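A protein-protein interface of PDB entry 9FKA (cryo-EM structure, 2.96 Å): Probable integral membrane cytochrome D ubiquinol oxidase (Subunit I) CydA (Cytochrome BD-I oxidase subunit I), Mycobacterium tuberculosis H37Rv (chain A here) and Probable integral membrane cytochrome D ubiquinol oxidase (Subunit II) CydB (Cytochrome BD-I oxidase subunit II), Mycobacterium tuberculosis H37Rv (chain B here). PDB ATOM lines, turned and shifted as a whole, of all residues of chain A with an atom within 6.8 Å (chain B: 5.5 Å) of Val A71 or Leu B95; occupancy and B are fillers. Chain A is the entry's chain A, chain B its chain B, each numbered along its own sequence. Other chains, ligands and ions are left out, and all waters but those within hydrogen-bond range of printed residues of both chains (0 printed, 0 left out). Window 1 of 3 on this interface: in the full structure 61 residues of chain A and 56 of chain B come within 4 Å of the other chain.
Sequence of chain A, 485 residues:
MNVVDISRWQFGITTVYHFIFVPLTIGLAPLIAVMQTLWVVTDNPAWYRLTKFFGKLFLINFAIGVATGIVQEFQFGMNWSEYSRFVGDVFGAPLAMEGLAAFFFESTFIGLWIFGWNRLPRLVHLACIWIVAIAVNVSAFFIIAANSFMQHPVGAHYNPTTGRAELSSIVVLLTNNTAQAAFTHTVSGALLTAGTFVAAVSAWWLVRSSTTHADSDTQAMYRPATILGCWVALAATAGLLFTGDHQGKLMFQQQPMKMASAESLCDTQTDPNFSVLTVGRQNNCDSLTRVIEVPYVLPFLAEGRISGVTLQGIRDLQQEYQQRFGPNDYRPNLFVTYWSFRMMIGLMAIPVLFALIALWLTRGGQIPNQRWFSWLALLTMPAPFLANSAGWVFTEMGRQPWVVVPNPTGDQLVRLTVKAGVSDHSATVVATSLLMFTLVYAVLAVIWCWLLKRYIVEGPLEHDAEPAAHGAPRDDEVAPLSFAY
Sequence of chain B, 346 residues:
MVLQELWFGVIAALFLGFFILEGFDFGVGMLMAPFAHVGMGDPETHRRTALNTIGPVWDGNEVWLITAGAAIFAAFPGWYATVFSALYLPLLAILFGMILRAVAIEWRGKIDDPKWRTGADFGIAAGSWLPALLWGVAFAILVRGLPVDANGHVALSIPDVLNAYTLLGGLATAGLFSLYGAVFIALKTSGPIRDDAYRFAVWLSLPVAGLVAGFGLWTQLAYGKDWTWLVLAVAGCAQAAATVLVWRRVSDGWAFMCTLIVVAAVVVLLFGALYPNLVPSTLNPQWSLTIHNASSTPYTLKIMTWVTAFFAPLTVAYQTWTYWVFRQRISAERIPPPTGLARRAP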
ATOM      1  N   GLN A  10     -15.345 -24.159   5.077  1.00  0.00           N
ATOM      2  CA  GLN A  10     -15.361 -23.514   6.384  1.00  0.00           C
ATOM      3  C   GLN A  10     -14.414 -22.326   6.412  1.00  0.00           C
ATOM      4  O   GLN A  10     -14.776 -21.241   6.879  1.00  0.00           O
ATOM      5  CB  GLN A  10     -14.989 -24.521   7.470  1.00  0.00           C
ATOM      6  CG  GLN A  10     -15.316 -24.052   8.877  1.00  0.00           C
ATOM      7  CD  GLN A  10     -14.325 -24.556   9.902  1.00  0.00           C
ATOM      8  OE1 GLN A  10     -14.067 -25.755   9.996  1.00  0.00           O
ATOM      9  NE2 GLN A  10     -13.763 -23.641  10.682  1.00  0.00           N
ATOM     10  N   THR A  14     -15.751 -18.509   6.876  1.00  0.00           N
ATOM     11  CA  THR A  14     -15.343 -17.786   8.072  1.00  0.00           C
ATOM     12  C   THR A  14     -14.449 -16.599   7.755  1.00  0.00           C
ATOM     13  O   THR A  14     -14.383 -15.664   8.558  1.00  0.00           O
ATOM     14  CB  THR A  14     -14.619 -18.720   9.040  1.00  0.00           C
ATOM     15  OG1 THR A  14     -13.478 -19.295   8.393  1.00  0.00           O
ATOM     16  CG2 THR A  14     -15.548 -19.823   9.515  1.00  0.00           C
ATOM     17  N   VAL A  66     -13.577  -7.519  15.128  1.00  0.00           N
ATOM     18  CA  VAL A  66     -12.697  -8.266  16.019  1.00  0.00           C
ATOM     19  C   VAL A  66     -13.275  -9.644  16.307  1.00  0.00           C
ATOM     20  O   VAL A  66     -12.541 -10.635  16.393  1.00  0.00           O
ATOM     21  CB  VAL A  66     -12.461  -7.474  17.318  1.00  0.00           C
ATOM     22  CG1 VAL A  66     -11.806  -8.357  18.366  1.00  0.00           C
ATOM     23  CG2 VAL A  66     -11.609  -6.250  17.041  1.00  0.00           C
ATOM     24  N   ALA A  67     -14.597  -9.732  16.463  1.00  0.00           N
ATOM     25  CA  ALA A  67     -15.217 -11.010  16.796  1.00  0.00           C
ATOM     26  C   ALA A  67     -14.966 -12.046  15.709  1.00  0.00           C
ATOM     27  O   ALA A  67     -14.657 -13.205  16.007  1.00  0.00           O
ATOM     28  CB  ALA A  67     -16.717 -10.822  17.015  1.00  0.00           C
ATOM     29  N   THR A  68     -15.096 -11.649  14.443  1.00  0.00           N
ATOM     30  CA  THR A  68     -14.912 -12.601  13.354  1.00  0.00           C
ATOM     31  C   THR A  68     -13.443 -12.941  13.144  1.00  0.00           C
ATOM     32  O   THR A  68     -13.126 -14.020  12.631  1.00  0.00           O
ATOM     33  CB  THR A  68     -15.507 -12.046  12.062  1.00  0.00           C
ATOM     34  OG1 THR A  68     -15.090 -10.688  11.883  1.00  0.00           O
ATOM     35  CG2 THR A  68     -17.024 -12.104  12.108  1.00  0.00           C
ATOM     36  N   GLY A  69     -12.535 -12.041  13.525  1.00  0.00           N
ATOM     37  CA  GLY A  69     -11.119 -12.284  13.314  1.00  0.00           C
ATOM     38  C   GLY A  69     -10.493 -13.254  14.290  1.00  0.00           C
ATOM     39  O   GLY A  69      -9.426 -13.802  13.998  1.00  0.00           O
ATOM     40  N   ILE A  70     -11.127 -13.480  15.440  1.00  0.00           N
ATOM     41  CA  ILE A  70     -10.552 -14.375  16.439  1.00  0.00           C
ATOM     42  C   ILE A  70     -10.462 -15.794  15.895  1.00  0.00           C
ATOM     43  O   ILE A  70      -9.455 -16.486  16.086  1.00  0.00           O
ATOM     44  CB  ILE A  70     -11.369 -14.319  17.741  1.00  0.00           C
ATOM     45  CG1 ILE A  70     -11.237 -12.943  18.391  1.00  0.00           C
ATOM     46  CG2 ILE A  70     -10.908 -15.397  18.703  1.00  0.00           C
ATOM     47  CD1 ILE A  70     -12.391 -12.587  19.295  1.00  0.00           C
ATOM     48  N   VAL A  71     -11.511 -16.253  15.211  1.00  0.00           N
ATOM     49  CA  VAL A  71     -11.529 -17.625  14.714  1.00  0.00           C
ATOM     50  C   VAL A  71     -10.387 -17.854  13.734  1.00  0.00           C
ATOM     51  O   VAL A  71      -9.719 -18.894  13.771  1.00  0.00           O
ATOM     52  CB  VAL A  71     -12.892 -17.943  14.074  1.00  0.00           C
ATOM     53  CG1 VAL A  71     -12.838 -19.276  13.350  1.00  0.00           C
ATOM     54  CG2 VAL A  71     -13.977 -17.956  15.132  1.00  0.00           C
ATOM     55  N   GLN A  72     -10.149 -16.892  12.841  1.00  0.00           N
ATOM     56  CA  GLN A  72      -9.109 -17.068  11.833  1.00  0.00           C
ATOM     57  C   GLN A  72      -7.754 -17.347  12.465  1.00  0.00           C
ATOM     58  O   GLN A  72      -6.931 -18.056  11.877  1.00  0.00           O
ATOM     59  CB  GLN A  72      -9.027 -15.827  10.944  1.00  0.00           C
ATOM     60  CG  GLN A  72     -10.351 -15.409  10.330  1.00  0.00           C
ATOM     61  CD  GLN A  72     -11.043 -16.544   9.610  1.00  0.00           C
ATOM     62  OE1 GLN A  72     -12.252 -16.728   9.737  1.00  0.00           O
ATOM     63  NE2 GLN A  72     -10.279 -17.313   8.845  1.00  0.00           N
ATOM     64  N   GLU A  73      -7.500 -16.802  13.656  1.00  0.00           N
ATOM     65  CA  GLU A  73      -6.196 -16.983  14.284  1.00  0.00           C
ATOM     66  C   GLU A  73      -5.913 -18.454  14.556  1.00  0.00           C
ATOM     67  O   GLU A  73      -4.799 -18.933  14.315  1.00  0.00           O
ATOM     68  CB  GLU A  73      -6.124 -16.178  15.581  1.00  0.00           C
ATOM     69  CG  GLU A  73      -4.825 -16.349  16.351  1.00  0.00           C
ATOM     70  CD  GLU A  73      -3.603 -16.015  15.519  1.00  0.00           C
ATOM     71  OE1 GLU A  73      -3.644 -15.013  14.777  1.00  0.00           O
ATOM     72  OE2 GLU A  73      -2.601 -16.755  15.608  1.00  0.00           O
ATOM     73  N   PHE A  74      -6.904 -19.185  15.060  1.00  0.00           N
ATOM     74  CA  PHE A  74      -6.712 -20.585  15.412  1.00  0.00           C
ATOM     75  C   PHE A  74      -7.053 -21.539  14.280  1.00  0.00           C
ATOM     76  O   PHE A  74      -6.644 -22.705  14.330  1.00  0.00           O
ATOM     77  CB  PHE A  74      -7.564 -20.943  16.634  1.00  0.00           C
ATOM     78  CG  PHE A  74      -7.387 -20.005  17.792  1.00  0.00           C
ATOM     79  CD1 PHE A  74      -6.151 -19.453  18.074  1.00  0.00           C
ATOM     80  CD2 PHE A  74      -8.458 -19.681  18.603  1.00  0.00           C
ATOM     81  CE1 PHE A  74      -5.988 -18.592  19.140  1.00  0.00           C
ATOM     82  CE2 PHE A  74      -8.303 -18.822  19.669  1.00  0.00           C
ATOM     83  CZ  PHE A  74      -7.066 -18.276  19.938  1.00  0.00           C
ATOM     84  N   GLN A  75      -7.813 -21.079  13.287  1.00  0.00           N
ATOM     85  CA  GLN A  75      -8.272 -22.006  12.219  1.00  0.00           C
ATOM     86  C   GLN A  75      -7.080 -22.756  11.610  1.00  0.00           C
ATOM     87  O   GLN A  75      -7.240 -23.957  11.309  1.00  0.00           O
ATOM     88  CB  GLN A  75      -9.040 -21.265  11.126  1.00  0.00           C
ATOM     89  CG  GLN A  75     -10.183 -22.075  10.526  1.00  0.00           C
ATOM     90  CD  GLN A  75     -11.328 -21.212  10.046  1.00  0.00           C
ATOM     91  OE1 GLN A  75     -12.486 -21.405  10.430  1.00  0.00           O
ATOM     92  NE2 GLN A  75     -11.013 -20.244   9.202  1.00  0.00           N
ATOM     93  N   PHE A  76      -5.937 -22.092  11.439  1.00  0.00           N
ATOM     94  CA  PHE A  76      -4.811 -22.739  10.773  1.00  0.00           C
ATOM     95  C   PHE A  76      -4.469 -24.063  11.443  1.00  0.00           C
ATOM     96  O   PHE A  76      -4.362 -25.100  10.780  1.00  0.00           O
ATOM     97  CB  PHE A  76      -3.597 -21.811  10.777  1.00  0.00           C
ATOM     98  CG  PHE A  76      -3.778 -20.576   9.950  1.00  0.00           C
ATOM     99  CD1 PHE A  76      -3.724 -20.639   8.570  1.00  0.00           C
ATOM    100  CD2 PHE A  76      -3.998 -19.352  10.550  1.00  0.00           C
ATOM    101  CE1 PHE A  76      -3.889 -19.506   7.807  1.00  0.00           C
ATOM    102  CE2 PHE A  76      -4.165 -18.215   9.791  1.00  0.00           C
ATOM    103  CZ  PHE A  76      -4.109 -18.292   8.419  1.00  0.00           C
ATOM    104  N   MET A  78      -6.346 -25.757  13.658  1.00  0.00           N
ATOM    105  CA  MET A  78      -7.489 -26.644  13.835  1.00  0.00           C
ATOM    106  C   MET A  78      -7.697 -27.530  12.613  1.00  0.00           C
ATOM    107  O   MET A  78      -7.788 -28.758  12.730  1.00  0.00           O
ATOM    108  CB  MET A  78      -8.747 -25.824  14.118  1.00  0.00           C
ATOM    109  CG  MET A  78      -8.610 -24.862  15.284  1.00  0.00           C
ATOM    110  SD  MET A  78     -10.060 -24.843  16.352  1.00  0.00           S
ATOM    111  CE  MET A  78     -11.183 -23.852  15.371  1.00  0.00           C
ATOM    112  N   MET A 436     -21.804 -24.446  12.945  1.00  0.00           N
ATOM    113  CA  MET A 436     -21.763 -23.546  14.092  1.00  0.00           C
ATOM    114  C   MET A 436     -21.318 -22.150  13.678  1.00  0.00           C
ATOM    115  O   MET A 436     -21.918 -21.148  14.080  1.00  0.00           O
ATOM    116  CB  MET A 436     -20.832 -24.112  15.164  1.00  0.00           C
ATOM    117  CG  MET A 436     -20.923 -23.400  16.502  1.00  0.00           C
ATOM    118  SD  MET A 436     -19.332 -23.302  17.341  1.00  0.00           S
ATOM    119  CE  MET A 436     -18.814 -21.650  16.890  1.00  0.00           C
ATOM    120  N   PHE A 437     -20.261 -22.063  12.868  1.00  0.00           N
ATOM    121  CA  PHE A 437     -19.775 -20.755  12.442  1.00  0.00           C
ATOM    122  C   PHE A 437     -20.729 -20.104  11.452  1.00  0.00           C
ATOM    123  O   PHE A 437     -20.958 -18.891  11.510  1.00  0.00           O
ATOM    124  CB  PHE A 437     -18.380 -20.885  11.831  1.00  0.00           C
ATOM    125  CG  PHE A 437     -17.291 -21.106  12.841  1.00  0.00           C
ATOM    126  CD1 PHE A 437     -17.204 -20.318  13.974  1.00  0.00           C
ATOM    127  CD2 PHE A 437     -16.350 -22.104  12.654  1.00  0.00           C
ATOM    128  CE1 PHE A 437     -16.205 -20.520  14.901  1.00  0.00           C
ATOM    129  CE2 PHE A 437     -15.348 -22.310  13.579  1.00  0.00           C
ATOM    130  CZ  PHE A 437     -15.275 -21.518  14.704  1.00  0.00           C
ATOM    131  N   TYR A 441     -22.345 -16.625  12.589  1.00  0.00           N
ATOM    132  CA  TYR A 441     -21.884 -15.470  11.829  1.00  0.00           C
ATOM    133  C   TYR A 441     -23.017 -14.853  11.023  1.00  0.00           C
ATOM    134  O   TYR A 441     -23.084 -13.630  10.885  1.00  0.00           O
ATOM    135  CB  TYR A 441     -20.728 -15.862  10.909  1.00  0.00           C
ATOM    136  CG  TYR A 441     -19.363 -15.888  11.569  1.00  0.00           C
ATOM    137  CD1 TYR A 441     -19.207 -15.629  12.926  1.00  0.00           C
ATOM    138  CD2 TYR A 441     -18.226 -16.162  10.827  1.00  0.00           C
ATOM    139  CE1 TYR A 441     -17.964 -15.650  13.518  1.00  0.00           C
ATOM    140  CE2 TYR A 441     -16.979 -16.184  11.411  1.00  0.00           C
ATOM    141  CZ  TYR A 441     -16.853 -15.927  12.756  1.00  0.00           C
ATOM    142  OH  TYR A 441     -15.610 -15.949  13.340  1.00  0.00           O
ATOM    143  N   LEU B  91     -11.726 -26.412  21.886  1.00  0.00           N
ATOM    144  CA  LEU B  91     -11.413 -25.062  21.432  1.00  0.00           C
ATOM    145  C   LEU B  91     -12.570 -24.442  20.663  1.00  0.00           C
ATOM    146  O   LEU B  91     -12.693 -23.212  20.620  1.00  0.00           O
ATOM    147  CB  LEU B  91     -10.156 -25.082  20.561  1.00  0.00           C
ATOM    148  CG  LEU B  91      -9.250 -23.847  20.581  1.00  0.00           C
ATOM    149  CD1 LEU B  91      -8.847 -23.453  21.994  1.00  0.00           C
ATOM    150  CD2 LEU B  91      -8.021 -24.102  19.728  1.00  0.00           C
ATOM    151  N   LEU B  92     -13.423 -25.264  20.049  1.00  0.00           N
ATOM    152  CA  LEU B  92     -14.563 -24.721  19.320  1.00  0.00           C
ATOM    153  C   LEU B  92     -15.503 -23.970  20.253  1.00  0.00           C
ATOM    154  O   LEU B  92     -15.984 -22.881  19.920  1.00  0.00           O
ATOM    155  CB  LEU B  92     -15.309 -25.845  18.600  1.00  0.00           C
ATOM    156  CG  LEU B  92     -16.240 -25.413  17.465  1.00  0.00           C
ATOM    157  CD1 LEU B  92     -15.447 -24.862  16.291  1.00  0.00           C
ATOM    158  CD2 LEU B  92     -17.121 -26.568  17.021  1.00  0.00           C
ATOM    159  N   ALA B  93     -15.776 -24.536  21.430  1.00  0.00           N
ATOM    160  CA  ALA B  93     -16.644 -23.862  22.390  1.00  0.00           C
ATOM    161  C   ALA B  93     -16.015 -22.565  22.883  1.00  0.00           C
ATOM    162  O   ALA B  93     -16.708 -21.553  23.047  1.00  0.00           O
ATOM    163  CB  ALA B  93     -16.948 -24.793  23.560  1.00  0.00           C
ATOM    164  N   ILE B  94     -14.704 -22.576  23.132  1.00  0.00           N
ATOM    165  CA  ILE B  94     -14.024 -21.355  23.553  1.00  0.00           C
ATOM    166  C   ILE B  94     -14.174 -20.278  22.489  1.00  0.00           C
ATOM    167  O   ILE B  94     -14.431 -19.108  22.798  1.00  0.00           O
ATOM    168  CB  ILE B  94     -12.542 -21.642  23.853  1.00  0.00           C
ATOM    169  CG1 ILE B  94     -12.410 -22.532  25.089  1.00  0.00           C
ATOM    170  CG2 ILE B  94     -11.784 -20.340  24.053  1.00  0.00           C
ATOM    171  CD1 ILE B  94     -11.045 -23.163  25.240  1.00  0.00           C
ATOM    172  N   LEU B  95     -14.004 -20.652  21.220  1.00  0.00           N
ATOM    173  CA  LEU B  95     -14.162 -19.687  20.139  1.00  0.00           C
ATOM    174  C   LEU B  95     -15.587 -19.158  20.079  1.00  0.00           C
ATOM    175  O   LEU B  95     -15.803 -17.965  19.850  1.00  0.00           O
ATOM    176  CB  LEU B  95     -13.770 -20.326  18.808  1.00  0.00           C
ATOM    177  CG  LEU B  95     -12.270 -20.371  18.520  1.00  0.00           C
ATOM    178  CD1 LEU B  95     -11.987 -21.213  17.290  1.00  0.00           C
ATOM    179  CD2 LEU B  95     -11.717 -18.968  18.350  1.00  0.00           C
ATOM    180  N   PHE B  96     -16.575 -20.033  20.271  1.00  0.00           N
ATOM    181  CA  PHE B  96     -17.966 -19.596  20.278  1.00  0.00           C
ATOM    182  C   PHE B  96     -18.208 -18.569  21.378  1.00  0.00           C
ATOM    183  O   PHE B  96     -18.812 -17.511  21.145  1.00  0.00           O
ATOM    184  CB  PHE B  96     -18.874 -20.815  20.452  1.00  0.00           C
ATOM    185  CG  PHE B  96     -20.322 -20.483  20.651  1.00  0.00           C
ATOM    186  CD1 PHE B  96     -21.159 -20.300  19.566  1.00  0.00           C
ATOM    187  CD2 PHE B  96     -20.854 -20.382  21.924  1.00  0.00           C
ATOM    188  CE1 PHE B  96     -22.496 -20.006  19.747  1.00  0.00           C
ATOM    189  CE2 PHE B  96     -22.189 -20.090  22.110  1.00  0.00           C
ATOM    190  CZ  PHE B  96     -23.011 -19.903  21.020  1.00  0.00           C
ATOM    191  N   GLY B  97     -17.725 -18.857  22.587  1.00  0.00           N
ATOM    192  CA  GLY B  97     -17.897 -17.917  23.680  1.00  0.00           C
ATOM    193  C   GLY B  97     -17.200 -16.596  23.427  1.00  0.00           C
ATOM    194  O   GLY B  97     -17.757 -15.528  23.693  1.00  0.00           O
ATOM    195  N   MET B  98     -15.972 -16.647  22.908  1.00  0.00           N
ATOM    196  CA  MET B  98     -15.244 -15.415  22.627  1.00  0.00           C
ATOM    197  C   MET B  98     -15.942 -14.597  21.551  1.00  0.00           C
ATOM    198  O   MET B  98     -16.004 -13.365  21.641  1.00  0.00           O
ATOM    199  CB  MET B  98     -13.811 -15.737  22.207  1.00  0.00           C
ATOM    200  CG  MET B  98     -12.836 -15.817  23.364  1.00  0.00           C
ATOM    201  SD  MET B  98     -11.278 -16.584  22.892  1.00  0.00           S
ATOM    202  CE  MET B  98     -10.282 -15.131  22.575  1.00  0.00           C
ATOM    203  N   ILE B  99     -16.470 -15.259  20.522  1.00  0.00           N
ATOM    204  CA  ILE B  99     -17.198 -14.552  19.474  1.00  0.00           C
ATOM    205  C   ILE B  99     -18.413 -13.855  20.065  1.00  0.00           C
ATOM    206  O   ILE B  99     -18.680 -12.683  19.778  1.00  0.00           O
ATOM    207  CB  ILE B  99     -17.603 -15.524  18.352  1.00  0.00           C
ATOM    208  CG1 ILE B  99     -16.366 -16.065  17.637  1.00  0.00           C
ATOM    209  CG2 ILE B  99     -18.518 -14.833  17.358  1.00  0.00           C
ATOM    210  CD1 ILE B  99     -16.571 -17.435  17.032  1.00  0.00           C
ATOM    211  N   LEU B 100     -19.171 -14.567  20.901  1.00  0.00           N
ATOM    212  CA  LEU B 100     -20.358 -13.956  21.491  1.00  0.00           C
ATOM    213  C   LEU B 100     -19.989 -12.778  22.386  1.00  0.00           C
ATOM    214  O   LEU B 100     -20.658 -11.740  22.361  1.00  0.00           O
ATOM    215  CB  LEU B 100     -21.157 -14.994  22.276  1.00  0.00           C
ATOM    216  CG  LEU B 100     -21.958 -16.014  21.465  1.00  0.00           C
ATOM    217  CD1 LEU B 100     -22.834 -16.835  22.394  1.00  0.00           C
ATOM    218  CD2 LEU B 100     -22.803 -15.345  20.392  1.00  0.00           C
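Val A71 touches just these residues of chain B: Leu B95 and Ile B99. Printed residues of chain B within 4 Å of Met A436: Leu B92 and Phe B96. Of the printed residues of chain B, Met A78 touches Leu B95. Leu B91 touches none of the printed residues of chain A. Ala B93 touches none of the printed residues of chain A. The nearest residue of chain A that does not touch Leu B95 is Phe A437 (4.2 Å). The nearest printed residue of chain B that does not touch Phe A74 is Leu B91 (4.4 Å).
Hydrophobic or aromatic side chains of chain B within 4 Å of the printed part of chain A: Leu B92, Leu B95, Phe B96, Met B98 and Ile B99. Along chain B the printed residues that touch a printed residue of chain A span positions 92 to 99. Printed residues of chain A that touch a printed residue of chain B: Ala A67, Ile A70, Val A71, Phe A74, Met A78, Met A436, Phe A437 and Tyr A441. Hydrophobic or aromatic side chains of chain A that line the printed part of chain B: Ala A67, Ile A70, Val A71, Phe A74, Met A78, Met A436, Phe A437 and Tyr A441. Among the printed residues, 12 pairs touch across the chains.
Among the printed residues, pairs that only touch across the chains: Ala A67 with Ile B99 (3.7 Å), Ile A70 with Leu B95 (3.7 Å), Ile A70 with Met B98 (3.9 Å), Val A71 with Leu B95 (3.9 Å), Val A71 with Ile B99 (3.3 Å), Phe A74 with Leu B95 (3.3 Å), Met A78 with Leu B95 (3.4 Å), Met A436 with Leu B92 (3.7 Å), Met A436 with Phe B96 (3.7 Å), Phe A437 with Leu B92 (3.7 Å), Phe A437 with Ile B99 (3.8 Å) and Tyr A441 with Ile B99 (3.96 Å).
The side-chain hydroxyl of Tyr A441 lies within hydrogen-bond range of the backbone carbonyl oxygen of Thr A68 (3.2 Å).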
